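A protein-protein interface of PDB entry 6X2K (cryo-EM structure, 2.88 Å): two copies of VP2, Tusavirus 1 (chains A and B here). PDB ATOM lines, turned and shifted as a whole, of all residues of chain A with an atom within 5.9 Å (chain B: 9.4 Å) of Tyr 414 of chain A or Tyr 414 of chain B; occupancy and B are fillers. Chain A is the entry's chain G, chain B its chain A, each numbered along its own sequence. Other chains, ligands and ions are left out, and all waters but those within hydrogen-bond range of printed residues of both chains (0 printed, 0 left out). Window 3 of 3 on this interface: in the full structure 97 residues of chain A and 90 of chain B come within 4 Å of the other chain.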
ATOM      1  N   TYR A 298     -13.422  20.699  -6.013  1.00  0.00           N
ATOM      2  CA  TYR A 298     -14.057  20.529  -7.308  1.00  0.00           C
ATOM      3  C   TYR A 298     -14.782  19.196  -7.346  1.00  0.00           C
ATOM      4  O   TYR A 298     -14.450  18.266  -6.609  1.00  0.00           O
ATOM      5  CB  TYR A 298     -13.029  20.636  -8.434  1.00  0.00           C
ATOM      6  CG  TYR A 298     -11.955  19.575  -8.434  1.00  0.00           C
ATOM      7  CD1 TYR A 298     -12.027  18.491  -9.281  1.00  0.00           C
ATOM      8  CD2 TYR A 298     -10.878  19.651  -7.576  1.00  0.00           C
ATOM      9  CE1 TYR A 298     -11.050  17.531  -9.286  1.00  0.00           C
ATOM     10  CE2 TYR A 298      -9.904  18.689  -7.573  1.00  0.00           C
ATOM     11  CZ  TYR A 298      -9.995  17.635  -8.430  1.00  0.00           C
ATOM     12  OH  TYR A 298      -9.022  16.675  -8.431  1.00  0.00           O
ATOM     13  N   ASN A 299     -15.785  19.120  -8.210  1.00  0.00           N
ATOM     14  CA  ASN A 299     -16.474  17.866  -8.468  1.00  0.00           C
ATOM     15  C   ASN A 299     -15.613  16.952  -9.317  1.00  0.00           C
ATOM     16  O   ASN A 299     -14.810  17.402 -10.129  1.00  0.00           O
ATOM     17  CB  ASN A 299     -17.795  18.105  -9.179  1.00  0.00           C
ATOM     18  CG  ASN A 299     -18.857  18.607  -8.263  1.00  0.00           C
ATOM     19  OD1 ASN A 299     -19.448  17.842  -7.512  1.00  0.00           O
ATOM     20  ND2 ASN A 299     -19.110  19.898  -8.310  1.00  0.00           N
ATOM     21  N   HIS A 300     -15.781  15.652  -9.114  1.00  0.00           N
ATOM     22  CA  HIS A 300     -15.021  14.693  -9.888  1.00  0.00           C
ATOM     23  C   HIS A 300     -15.858  13.439 -10.048  1.00  0.00           C
ATOM     24  O   HIS A 300     -16.671  13.125  -9.174  1.00  0.00           O
ATOM     25  CB  HIS A 300     -13.679  14.394  -9.208  1.00  0.00           C
ATOM     26  CG  HIS A 300     -12.683  13.705 -10.083  1.00  0.00           C
ATOM     27  ND1 HIS A 300     -12.585  12.336 -10.172  1.00  0.00           N
ATOM     28  CD2 HIS A 300     -11.754  14.203 -10.929  1.00  0.00           C
ATOM     29  CE1 HIS A 300     -11.626  12.021 -11.020  1.00  0.00           C
ATOM     30  NE2 HIS A 300     -11.108  13.135 -11.496  1.00  0.00           N
ATOM     31  N   ASN A 412     -17.611  16.979 -13.589  1.00  0.00           N
ATOM     32  CA  ASN A 412     -16.246  17.441 -13.374  1.00  0.00           C
ATOM     33  C   ASN A 412     -16.246  18.955 -13.472  1.00  0.00           C
ATOM     34  O   ASN A 412     -16.398  19.509 -14.562  1.00  0.00           O
ATOM     35  CB  ASN A 412     -15.292  16.818 -14.385  1.00  0.00           C
ATOM     36  CG  ASN A 412     -13.847  17.047 -14.036  1.00  0.00           C
ATOM     37  OD1 ASN A 412     -13.515  17.963 -13.303  1.00  0.00           O
ATOM     38  ND2 ASN A 412     -12.980  16.197 -14.540  1.00  0.00           N
ATOM     39  N   THR A 413     -16.070  19.623 -12.337  1.00  0.00           N
ATOM     40  CA  THR A 413     -16.038  21.073 -12.270  1.00  0.00           C
ATOM     41  C   THR A 413     -14.633  21.638 -12.153  1.00  0.00           C
ATOM     42  O   THR A 413     -14.487  22.830 -11.890  1.00  0.00           O
ATOM     43  CB  THR A 413     -16.911  21.577 -11.128  1.00  0.00           C
ATOM     44  OG1 THR A 413     -16.497  20.979  -9.901  1.00  0.00           O
ATOM     45  CG2 THR A 413     -18.354  21.238 -11.392  1.00  0.00           C
ATOM     46  N   TYR A 414     -13.605  20.813 -12.275  1.00  0.00           N
ATOM     47  CA  TYR A 414     -12.244  21.321 -12.211  1.00  0.00           C
ATOM     48  C   TYR A 414     -12.050  22.414 -13.250  1.00  0.00           C
ATOM     49  O   TYR A 414     -12.666  22.398 -14.315  1.00  0.00           O
ATOM     50  CB  TYR A 414     -11.251  20.195 -12.462  1.00  0.00           C
ATOM     51  CG  TYR A 414      -9.811  20.592 -12.250  1.00  0.00           C
ATOM     52  CD1 TYR A 414      -9.265  20.610 -10.997  1.00  0.00           C
ATOM     53  CD2 TYR A 414      -9.021  20.960 -13.310  1.00  0.00           C
ATOM     54  CE1 TYR A 414      -7.969  20.969 -10.798  1.00  0.00           C
ATOM     55  CE2 TYR A 414      -7.720  21.329 -13.116  1.00  0.00           C
ATOM     56  CZ  TYR A 414      -7.199  21.335 -11.866  1.00  0.00           C
ATOM     57  OH  TYR A 414      -5.890  21.703 -11.707  1.00  0.00           O
ATOM     58  N   GLY A 415     -11.212  23.385 -12.925  1.00  0.00           N
ATOM     59  CA  GLY A 415     -11.028  24.515 -13.808  1.00  0.00           C
ATOM     60  C   GLY A 415      -9.977  25.457 -13.278  1.00  0.00           C
ATOM     61  O   GLY A 415      -9.168  25.095 -12.426  1.00  0.00           O
ATOM     62  N   VAL A 416     -10.009  26.684 -13.789  1.00  0.00           N
ATOM     63  CA  VAL A 416      -8.942  27.636 -13.508  1.00  0.00           C
ATOM     64  C   VAL A 416      -9.069  28.226 -12.112  1.00  0.00           C
ATOM     65  O   VAL A 416      -8.068  28.616 -11.505  1.00  0.00           O
ATOM     66  CB  VAL A 416      -8.934  28.727 -14.590  1.00  0.00           C
ATOM     67  CG1 VAL A 416      -7.948  29.783 -14.268  1.00  0.00           C
ATOM     68  CG2 VAL A 416      -8.587  28.118 -15.916  1.00  0.00           C
ATOM     69  N   THR A 418     -10.042  26.706  -9.304  1.00  0.00           N
ATOM     70  CA  THR A 418     -10.121  25.739  -8.222  1.00  0.00           C
ATOM     71  C   THR A 418      -8.868  25.751  -7.357  1.00  0.00           C
ATOM     72  O   THR A 418      -7.759  26.000  -7.829  1.00  0.00           O
ATOM     73  CB  THR A 418     -10.341  24.338  -8.774  1.00  0.00           C
ATOM     74  OG1 THR A 418      -9.208  23.953  -9.543  1.00  0.00           O
ATOM     75  CG2 THR A 418     -11.540  24.333  -9.674  1.00  0.00           C
ATOM     76  N   LYS A 441       4.164  16.440 -17.853  1.00  0.00           N
ATOM     77  CA  LYS A 441       3.300  17.100 -16.890  1.00  0.00           C
ATOM     78  C   LYS A 441       3.397  16.375 -15.560  1.00  0.00           C
ATOM     79  O   LYS A 441       3.122  15.175 -15.483  1.00  0.00           O
ATOM     80  CB  LYS A 441       1.848  17.111 -17.344  1.00  0.00           C
ATOM     81  CG  LYS A 441       0.975  17.714 -16.285  1.00  0.00           C
ATOM     82  CD  LYS A 441      -0.469  17.739 -16.611  1.00  0.00           C
ATOM     83  CE  LYS A 441      -1.200  18.348 -15.444  1.00  0.00           C
ATOM     84  NZ  LYS A 441      -1.143  17.488 -14.250  1.00  0.00           N
ATOM     85  N   GLU A 444      -0.063  17.788  -9.400  1.00  0.00           N
ATOM     86  CA  GLU A 444      -0.113  18.904  -8.473  1.00  0.00           C
ATOM     87  C   GLU A 444      -0.125  18.470  -7.016  1.00  0.00           C
ATOM     88  O   GLU A 444       0.129  19.300  -6.140  1.00  0.00           O
ATOM     89  CB  GLU A 444      -1.338  19.753  -8.782  1.00  0.00           C
ATOM     90  CG  GLU A 444      -1.266  20.405 -10.134  1.00  0.00           C
ATOM     91  CD  GLU A 444      -2.583  20.981 -10.576  1.00  0.00           C
ATOM     92  OE1 GLU A 444      -3.604  20.672  -9.941  1.00  0.00           O
ATOM     93  OE2 GLU A 444      -2.609  21.733 -11.562  1.00  0.00           O
ATOM     94  N   THR B 295      -2.406   9.364 -10.766  1.00  0.00           N
ATOM     95  CA  THR B 295      -3.042   8.728 -11.908  1.00  0.00           C
ATOM     96  C   THR B 295      -2.318   9.157 -13.172  1.00  0.00           C
ATOM     97  O   THR B 295      -1.980  10.328 -13.330  1.00  0.00           O
ATOM     98  CB  THR B 295      -4.511   9.108 -12.031  1.00  0.00           C
ATOM     99  OG1 THR B 295      -4.598  10.475 -12.419  1.00  0.00           O
ATOM    100  CG2 THR B 295      -5.197   8.957 -10.707  1.00  0.00           C
ATOM    101  N   ALA B 296      -2.089   8.210 -14.069  1.00  0.00           N
ATOM    102  CA  ALA B 296      -1.441   8.482 -15.342  1.00  0.00           C
ATOM    103  C   ALA B 296      -2.497   8.689 -16.416  1.00  0.00           C
ATOM    104  O   ALA B 296      -3.363   7.835 -16.611  1.00  0.00           O
ATOM    105  CB  ALA B 296      -0.511   7.339 -15.734  1.00  0.00           C
ATOM    106  N   GLY B 297      -2.428   9.824 -17.103  1.00  0.00           N
ATOM    107  CA  GLY B 297      -3.371  10.116 -18.162  1.00  0.00           C
ATOM    108  C   GLY B 297      -4.746  10.442 -17.629  1.00  0.00           C
ATOM    109  O   GLY B 297      -4.981  10.350 -16.424  1.00  0.00           O
ATOM    110  N   TYR B 298      -5.668  10.825 -18.508  1.00  0.00           N
ATOM    111  CA  TYR B 298      -6.993  11.208 -18.054  1.00  0.00           C
ATOM    112  C   TYR B 298      -7.991  11.011 -19.180  1.00  0.00           C
ATOM    113  O   TYR B 298      -7.635  11.013 -20.359  1.00  0.00           O
ATOM    114  CB  TYR B 298      -6.998  12.653 -17.554  1.00  0.00           C
ATOM    115  CG  TYR B 298      -6.673  13.700 -18.592  1.00  0.00           C
ATOM    116  CD1 TYR B 298      -7.668  14.434 -19.198  1.00  0.00           C
ATOM    117  CD2 TYR B 298      -5.370  13.940 -18.978  1.00  0.00           C
ATOM    118  CE1 TYR B 298      -7.373  15.389 -20.135  1.00  0.00           C
ATOM    119  CE2 TYR B 298      -5.073  14.888 -19.921  1.00  0.00           C
ATOM    120  CZ  TYR B 298      -6.076  15.607 -20.492  1.00  0.00           C
ATOM    121  OH  TYR B 298      -5.782  16.555 -21.432  1.00  0.00           O
ATOM    122  N   ASN B 299      -9.249  10.828 -18.797  1.00  0.00           N
ATOM    123  CA  ASN B 299     -10.336  10.775 -19.761  1.00  0.00           C
ATOM    124  C   ASN B 299     -10.650  12.162 -20.285  1.00  0.00           C
ATOM    125  O   ASN B 299     -10.474  13.162 -19.593  1.00  0.00           O
ATOM    126  CB  ASN B 299     -11.590  10.187 -19.136  1.00  0.00           C
ATOM    127  CG  ASN B 299     -11.519   8.706 -18.995  1.00  0.00           C
ATOM    128  OD1 ASN B 299     -11.709   7.976 -19.960  1.00  0.00           O
ATOM    129  ND2 ASN B 299     -11.244   8.242 -17.794  1.00  0.00           N
ATOM    130  N   HIS B 300     -11.108  12.217 -21.527  1.00  0.00           N
ATOM    131  CA  HIS B 300     -11.456  13.494 -22.117  1.00  0.00           C
ATOM    132  C   HIS B 300     -12.579  13.270 -23.111  1.00  0.00           C
ATOM    133  O   HIS B 300     -12.670  12.191 -23.705  1.00  0.00           O
ATOM    134  CB  HIS B 300     -10.230  14.130 -22.784  1.00  0.00           C
ATOM    135  CG  HIS B 300     -10.386  15.582 -23.106  1.00  0.00           C
ATOM    136  ND1 HIS B 300     -10.883  16.033 -24.306  1.00  0.00           N
ATOM    137  CD2 HIS B 300     -10.132  16.685 -22.367  1.00  0.00           C
ATOM    138  CE1 HIS B 300     -10.909  17.352 -24.300  1.00  0.00           C
ATOM    139  NE2 HIS B 300     -10.461  17.772 -23.134  1.00  0.00           N
ATOM    140  N   PRO B 301     -13.472  14.242 -23.289  1.00  0.00           N
ATOM    141  CA  PRO B 301     -14.543  14.024 -24.271  1.00  0.00           C
ATOM    142  C   PRO B 301     -14.012  13.844 -25.697  1.00  0.00           C
ATOM    143  O   PRO B 301     -13.392  14.756 -26.224  1.00  0.00           O
ATOM    144  CB  PRO B 301     -15.354  15.309 -24.179  1.00  0.00           C
ATOM    145  CG  PRO B 301     -15.134  15.786 -22.787  1.00  0.00           C
ATOM    146  CD  PRO B 301     -13.730  15.406 -22.429  1.00  0.00           C
ATOM    147  N   ALA B 317      -7.220  15.603 -26.450  1.00  0.00           N
ATOM    148  CA  ALA B 317      -6.291  15.103 -25.451  1.00  0.00           C
ATOM    149  C   ALA B 317      -5.017  14.614 -26.133  1.00  0.00           C
ATOM    150  O   ALA B 317      -5.011  14.376 -27.335  1.00  0.00           O
ATOM    151  CB  ALA B 317      -6.942  13.984 -24.645  1.00  0.00           C
ATOM    152  N   PRO B 318      -3.915  14.460 -25.400  1.00  0.00           N
ATOM    153  CA  PRO B 318      -2.670  14.041 -26.033  1.00  0.00           C
ATOM    154  C   PRO B 318      -2.817  12.677 -26.680  1.00  0.00           C
ATOM    155  O   PRO B 318      -3.593  11.827 -26.211  1.00  0.00           O
ATOM    156  CB  PRO B 318      -1.681  13.998 -24.862  1.00  0.00           C
ATOM    157  CG  PRO B 318      -2.218  14.939 -23.898  1.00  0.00           C
ATOM    158  CD  PRO B 318      -3.696  14.803 -23.984  1.00  0.00           C
ATOM    159  N   ILE B 371      -5.815   4.842 -22.722  1.00  0.00           N
ATOM    160  CA  ILE B 371      -7.020   4.404 -22.037  1.00  0.00           C
ATOM    161  C   ILE B 371      -7.881   3.634 -23.018  1.00  0.00           C
ATOM    162  O   ILE B 371      -8.354   4.198 -24.010  1.00  0.00           O
ATOM    163  CB  ILE B 371      -7.809   5.583 -21.451  1.00  0.00           C
ATOM    164  CG1 ILE B 371      -7.031   6.225 -20.310  1.00  0.00           C
ATOM    165  CG2 ILE B 371      -9.161   5.131 -20.971  1.00  0.00           C
ATOM    166  CD1 ILE B 371      -7.629   7.495 -19.820  1.00  0.00           C
ATOM    167  N   PRO B 411     -16.570  11.344 -20.643  1.00  0.00           N
ATOM    168  CA  PRO B 411     -15.986  11.589 -19.326  1.00  0.00           C
ATOM    169  C   PRO B 411     -14.913  12.660 -19.377  1.00  0.00           C
ATOM    170  O   PRO B 411     -14.247  12.855 -20.389  1.00  0.00           O
ATOM    171  CB  PRO B 411     -15.394  10.226 -18.956  1.00  0.00           C
ATOM    172  CG  PRO B 411     -14.994   9.681 -20.228  1.00  0.00           C
ATOM    173  CD  PRO B 411     -15.954  10.162 -21.263  1.00  0.00           C
ATOM    174  N   ASN B 412     -14.740  13.361 -18.266  1.00  0.00           N
ATOM    175  CA  ASN B 412     -13.520  14.128 -18.051  1.00  0.00           C
ATOM    176  C   ASN B 412     -13.026  13.832 -16.646  1.00  0.00           C
ATOM    177  O   ASN B 412     -13.631  14.274 -15.667  1.00  0.00           O
ATOM    178  CB  ASN B 412     -13.769  15.618 -18.251  1.00  0.00           C
ATOM    179  CG  ASN B 412     -12.494  16.416 -18.308  1.00  0.00           C
ATOM    180  OD1 ASN B 412     -11.461  15.985 -17.826  1.00  0.00           O
ATOM    181  ND2 ASN B 412     -12.556  17.575 -18.924  1.00  0.00           N
ATOM    182  N   THR B 413     -11.928  13.092 -16.548  1.00  0.00           N
ATOM    183  CA  THR B 413     -11.329  12.732 -15.275  1.00  0.00           C
ATOM    184  C   THR B 413     -10.109  13.566 -14.928  1.00  0.00           C
ATOM    185  O   THR B 413      -9.402  13.227 -13.980  1.00  0.00           O
ATOM    186  CB  THR B 413     -10.985  11.248 -15.244  1.00  0.00           C
ATOM    187  OG1 THR B 413     -10.134  10.925 -16.343  1.00  0.00           O
ATOM    188  CG2 THR B 413     -12.244  10.425 -15.323  1.00  0.00           C
ATOM    189  N   TYR B 414      -9.805  14.599 -15.698  1.00  0.00           N
ATOM    190  CA  TYR B 414      -8.670  15.448 -15.374  1.00  0.00           C
ATOM    191  C   TYR B 414      -8.812  15.987 -13.960  1.00  0.00           C
ATOM    192  O   TYR B 414      -9.918  16.203 -13.469  1.00  0.00           O
ATOM    193  CB  TYR B 414      -8.584  16.607 -16.358  1.00  0.00           C
ATOM    194  CG  TYR B 414      -7.341  17.448 -16.204  1.00  0.00           C
ATOM    195  CD1 TYR B 414      -6.159  17.060 -16.770  1.00  0.00           C
ATOM    196  CD2 TYR B 414      -7.365  18.612 -15.480  1.00  0.00           C
ATOM    197  CE1 TYR B 414      -5.033  17.811 -16.634  1.00  0.00           C
ATOM    198  CE2 TYR B 414      -6.236  19.368 -15.334  1.00  0.00           C
ATOM    199  CZ  TYR B 414      -5.077  18.967 -15.906  1.00  0.00           C
ATOM    200  OH  TYR B 414      -3.966  19.749 -15.747  1.00  0.00           O
ATOM    201  N   GLY B 415      -7.684  16.175 -13.292  1.00  0.00           N
ATOM    202  CA  GLY B 415      -7.718  16.599 -11.910  1.00  0.00           C
ATOM    203  C   GLY B 415      -6.327  16.823 -11.374  1.00  0.00           C
ATOM    204  O   GLY B 415      -5.369  16.972 -12.129  1.00  0.00           O
ATOM    205  N   VAL B 416      -6.227  16.831 -10.049  1.00  0.00           N
ATOM    206  CA  VAL B 416      -4.984  17.220  -9.397  1.00  0.00           C
ATOM    207  C   VAL B 416      -3.948  16.109  -9.456  1.00  0.00           C
ATOM    208  O   VAL B 416      -2.743  16.378  -9.446  1.00  0.00           O
ATOM    209  CB  VAL B 416      -5.279  17.649  -7.951  1.00  0.00           C
ATOM    210  CG1 VAL B 416      -4.024  17.928  -7.216  1.00  0.00           C
ATOM    211  CG2 VAL B 416      -6.130  18.883  -7.956  1.00  0.00           C
ATOM    212  N   TYR B 417      -4.378  14.861  -9.552  1.00  0.00           N
ATOM    213  CA  TYR B 417      -3.473  13.726  -9.515  1.00  0.00           C
ATOM    214  C   TYR B 417      -2.941  13.317 -10.879  1.00  0.00           C
ATOM    215  O   TYR B 417      -2.149  12.378 -10.952  1.00  0.00           O
ATOM    216  CB  TYR B 417      -4.172  12.530  -8.879  1.00  0.00           C
ATOM    217  CG  TYR B 417      -4.496  12.694  -7.418  1.00  0.00           C
ATOM    218  CD1 TYR B 417      -3.631  13.345  -6.572  1.00  0.00           C
ATOM    219  CD2 TYR B 417      -5.649  12.166  -6.882  1.00  0.00           C
ATOM    220  CE1 TYR B 417      -3.916  13.485  -5.246  1.00  0.00           C
ATOM    221  CE2 TYR B 417      -5.938  12.301  -5.556  1.00  0.00           C
ATOM    222  CZ  TYR B 417      -5.068  12.959  -4.745  1.00  0.00           C
ATOM    223  OH  TYR B 417      -5.345  13.095  -3.412  1.00  0.00           O
ATOM    224  N   THR B 418      -3.336  13.981 -11.954  1.00  0.00           N
ATOM    225  CA  THR B 418      -3.044  13.471 -13.283  1.00  0.00           C
ATOM    226  C   THR B 418      -1.643  13.853 -13.743  1.00  0.00           C
ATOM    227  O   THR B 418      -1.117  14.913 -13.403  1.00  0.00           O
ATOM    228  CB  THR B 418      -4.063  13.985 -14.289  1.00  0.00           C
ATOM    229  OG1 THR B 418      -3.948  15.399 -14.393  1.00  0.00           O
ATOM    230  CG2 THR B 418      -5.448  13.664 -13.812  1.00  0.00           C
ATOM    231  N   ALA B 419      -1.045  12.970 -14.535  1.00  0.00           N
ATOM    232  CA  ALA B 419       0.253  13.188 -15.149  1.00  0.00           C
ATOM    233  C   ALA B 419       0.233  12.602 -16.551  1.00  0.00           C
ATOM    234  O   ALA B 419      -0.264  11.493 -16.746  1.00  0.00           O
ATOM    235  CB  ALA B 419       1.359  12.543 -14.324  1.00  0.00           C
ATOM    236  N   VAL B 420       0.765  13.340 -17.529  1.00  0.00           N
ATOM    237  CA  VAL B 420       0.723  12.922 -18.925  1.00  0.00           C
ATOM    238  C   VAL B 420       2.088  13.142 -19.565  1.00  0.00           C
ATOM    239  O   VAL B 420       2.944  13.845 -19.035  1.00  0.00           O
ATOM    240  CB  VAL B 420      -0.353  13.672 -19.739  1.00  0.00           C
ATOM    241  CG1 VAL B 420      -1.714  13.500 -19.125  1.00  0.00           C
ATOM    242  CG2 VAL B 420      -0.008  15.120 -19.866  1.00  0.00           C
ATOM    243  N   LYS B 441      -3.181  32.306 -18.626  1.00  0.00           N
ATOM    244  CA  LYS B 441      -2.890  30.904 -18.379  1.00  0.00           C
ATOM    245  C   LYS B 441      -2.230  30.311 -19.610  1.00  0.00           C
ATOM    246  O   LYS B 441      -2.805  30.342 -20.700  1.00  0.00           O
ATOM    247  CB  LYS B 441      -4.148  30.111 -18.059  1.00  0.00           C
ATOM    248  CG  LYS B 441      -3.823  28.656 -17.904  1.00  0.00           C
ATOM    249  CD  LYS B 441      -4.987  27.784 -17.628  1.00  0.00           C
ATOM    250  CE  LYS B 441      -4.494  26.366 -17.525  1.00  0.00           C
ATOM    251  NZ  LYS B 441      -3.999  25.860 -18.816  1.00  0.00           N
ATOM    252  N   LYS B 442      -1.067  29.763 -19.432  1.00  0.00           N
ATOM    253  CA  LYS B 442      -0.390  29.086 -20.514  1.00  0.00           C
ATOM    254  C   LYS B 442      -0.779  27.618 -20.560  1.00  0.00           C
ATOM    255  O   LYS B 442      -1.256  27.057 -19.577  1.00  0.00           O
ATOM    256  CB  LYS B 442       1.114  29.212 -20.347  1.00  0.00           C
ATOM    257  CG  LYS B 442       1.733  30.395 -21.057  1.00  0.00           C
ATOM    258  CD  LYS B 442       1.397  31.713 -20.429  1.00  0.00           C
ATOM    259  CE  LYS B 442       2.109  32.819 -21.178  1.00  0.00           C
ATOM    260  NZ  LYS B 442       1.854  34.142 -20.565  1.00  0.00           N
ATOM    261  N   PRO B 443      -0.627  26.976 -21.709  1.00  0.00           N
ATOM    262  CA  PRO B 443      -0.837  25.532 -21.784  1.00  0.00           C
ATOM    263  C   PRO B 443       0.279  24.777 -21.088  1.00  0.00           C
ATOM    264  O   PRO B 443       1.385  25.277 -20.897  1.00  0.00           O
ATOM    265  CB  PRO B 443      -0.826  25.250 -23.288  1.00  0.00           C
ATOM    266  CG  PRO B 443      -1.160  26.532 -23.894  1.00  0.00           C
ATOM    267  CD  PRO B 443      -0.539  27.569 -23.046  1.00  0.00           C
ATOM    268  N   GLU B 444      -0.026  23.542 -20.717  1.00  0.00           N
ATOM    269  CA  GLU B 444       0.952  22.659 -20.108  1.00  0.00           C
ATOM    270  C   GLU B 444       1.728  21.836 -21.124  1.00  0.00           C
ATOM    271  O   GLU B 444       2.771  21.277 -20.775  1.00  0.00           O
ATOM    272  CB  GLU B 444       0.247  21.745 -19.116  1.00  0.00           C
ATOM    273  CG  GLU B 444      -0.340  22.494 -17.954  1.00  0.00           C
ATOM    274  CD  GLU B 444      -1.293  21.659 -17.142  1.00  0.00           C
ATOM    275  OE1 GLU B 444      -1.676  20.577 -17.612  1.00  0.00           O
ATOM    276  OE2 GLU B 444      -1.673  22.083 -16.039  1.00  0.00           O
ATOM    277  N   LEU B 445       1.258  21.773 -22.364  1.00  0.00           N
ATOM    278  CA  LEU B 445       1.940  21.096 -23.457  1.00  0.00           C
ATOM    279  C   LEU B 445       1.464  21.729 -24.752  1.00  0.00           C
ATOM    280  O   LEU B 445       0.466  22.444 -24.778  1.00  0.00           O
ATOM    281  CB  LEU B 445       1.665  19.590 -23.471  1.00  0.00           C
ATOM    282  CG  LEU B 445       2.164  18.651 -22.376  1.00  0.00           C
ATOM    283  CD1 LEU B 445       1.615  17.274 -22.620  1.00  0.00           C
ATOM    284  CD2 LEU B 445       3.669  18.602 -22.333  1.00  0.00           C
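The backbone carbonyl oxygen (O) of Val 420 of chain B sits at hydrogen-bond distance from the backbone NH (N) of Lys 441 of chain A (3.1 Å).
The backbone carbonyl oxygen of Tyr 414 of chain B is in hydrogen-bond range of the side-chain amide nitrogen of Asn 412 of chain A.
The side-chain amide nitrogen (ND2) of Asn 412 of chain A lies close to the backbone carbonyl oxygen (O) of Asn 412 of chain B (2.3 Å).
O of Val 416 of chain B sits at hydrogen-bond distance from N of Glu 444 of chain A, 3.0 Å away.
The backbone carbonyl oxygen (O) of Thr 418 of chain B lies within hydrogen-bond range of the side-chain amino group (NZ) of Lys 441 of chain A (2.7 Å).
The backbone carbonyl oxygen (O) of Thr 413 of chain B sits at hydrogen-bond distance from a ring nitrogen (NE2) of His 300 of chain A (3.0 Å).
N of Val 416 of chain B is in hydrogen-bond range of OH of Tyr 298 of chain A, at 3.2 Å.
The side-chain amide oxygen of Asn 412 of chain B is in hydrogen-bond range of the backbone NH of Tyr 414 of chain B (3.0 Å).
The side-chain carboxylate (OE1) of Glu 444 of chain A lies within hydrogen-bond range of the side-chain hydroxyl (OH) of Tyr 414 of chain A, 3.1 Å away.
O of Gly 415 of chain B sits at hydrogen-bond distance from OG1 of Thr 418 of chain B (3.1 Å).
O of Asn 299 of chain B lies close to OD1 of Asn 412 of chain B (3.5 Å).
O of Ala 419 of chain B sits at hydrogen-bond distance from N of Gly 297 of chain B (2.8 Å).
The backbone carbonyl oxygen (O) of Asn 299 of chain A sits close to the side-chain amide oxygen (OD1) of Asn 412 of chain A.
Among the printed residues, merely in contact across the chains: Lys 441 of chain A with Tyr 414 of chain B (3.1 Å), Lys 441 of chain A with Glu 444 of chain B (3.1 Å), Tyr 414 of chain A with Tyr 414 of chain B (3.3 Å), Lys 441 of chain A with Ala 419 of chain B (3.4 Å), Tyr 298 of chain A with Gly 415 of chain B (3.7 Å), His 300 of chain A with Tyr 414 of chain B (3.7 Å), Asn 412 of chain A with Thr 413 of chain B (3.8 Å) and Tyr 414 of chain A with Val 416 of chain B (3.98 Å).
Printed residues of chain B within 4 Å of Asn 412 of chain A: Asn 412 (2.3 Å), Thr 413 (3.8 Å) and Tyr 414 (3.2 Å).
Tyr 414 of chain A touches just these residues of chain B: Tyr 414 (3.3 Å) and Val 416 (3.98 Å).
No residue of chain B comes within 4 Å of Gly 415 of chain A.
Pro 411 of chain B touches none of the printed residues of chain A.
Of chain A, only His 300, Asn 412, Tyr 414 and Lys 441 come within 4 Å of Tyr 414 of chain B.
Printed residues of chain A within 4 Å of Val 416 of chain B: Tyr 298, Tyr 414 and Glu 444.
The nearest residue of chain B that does not touch Tyr 414 of chain A is Gly 415 of chain B (4.4 Å).
Printed residues of chain B that touch a printed residue of chain A: Asn 412, Thr 413, Tyr 414, Gly 415, Val 416, Thr 418, Ala 419, Val 420 and Glu 444.
Hydrophobic or aromatic side chains of chain B within 4 Å of the printed part of chain A: Tyr 414, Val 416, Ala 419 and Val 420.
Of the 11 printed residues of chain A, 6 touch a printed residue of chain B.
Printed residues of chain A that touch a printed residue of chain B: Tyr 298, His 300, Asn 412, Tyr 414, Lys 441 and Glu 444.
Among the printed residues, 15 pairs touch across the chains.
Among the printed residues, no Asp or Glu carboxylate lies within 4 Å of a Lys or Arg side-chain nitrogen of the other chain.
Tyr 298 of chain A touches Val 416 of chain B, but with the chains exchanged Val 416 of chain A does not touch Tyr 298 of chain B (13.1 Å).
His 300 of chain A touches Tyr 414 of chain B, but with the chains exchanged Tyr 414 of chain A does not touch His 300 of chain B (10.1 Å).
Tyr 414 of chain B touches its own counterpart, Tyr 414 of chain A.
Lys 441 of chain A touches Tyr 414 of chain B, but with the chains exchanged Tyr 414 of chain A does not touch Lys 441 of chain B (7.4 Å).
Of the 15 pairs that touch across the chains among the printed residues, 2 have their exchanged pair printed and touching as well.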
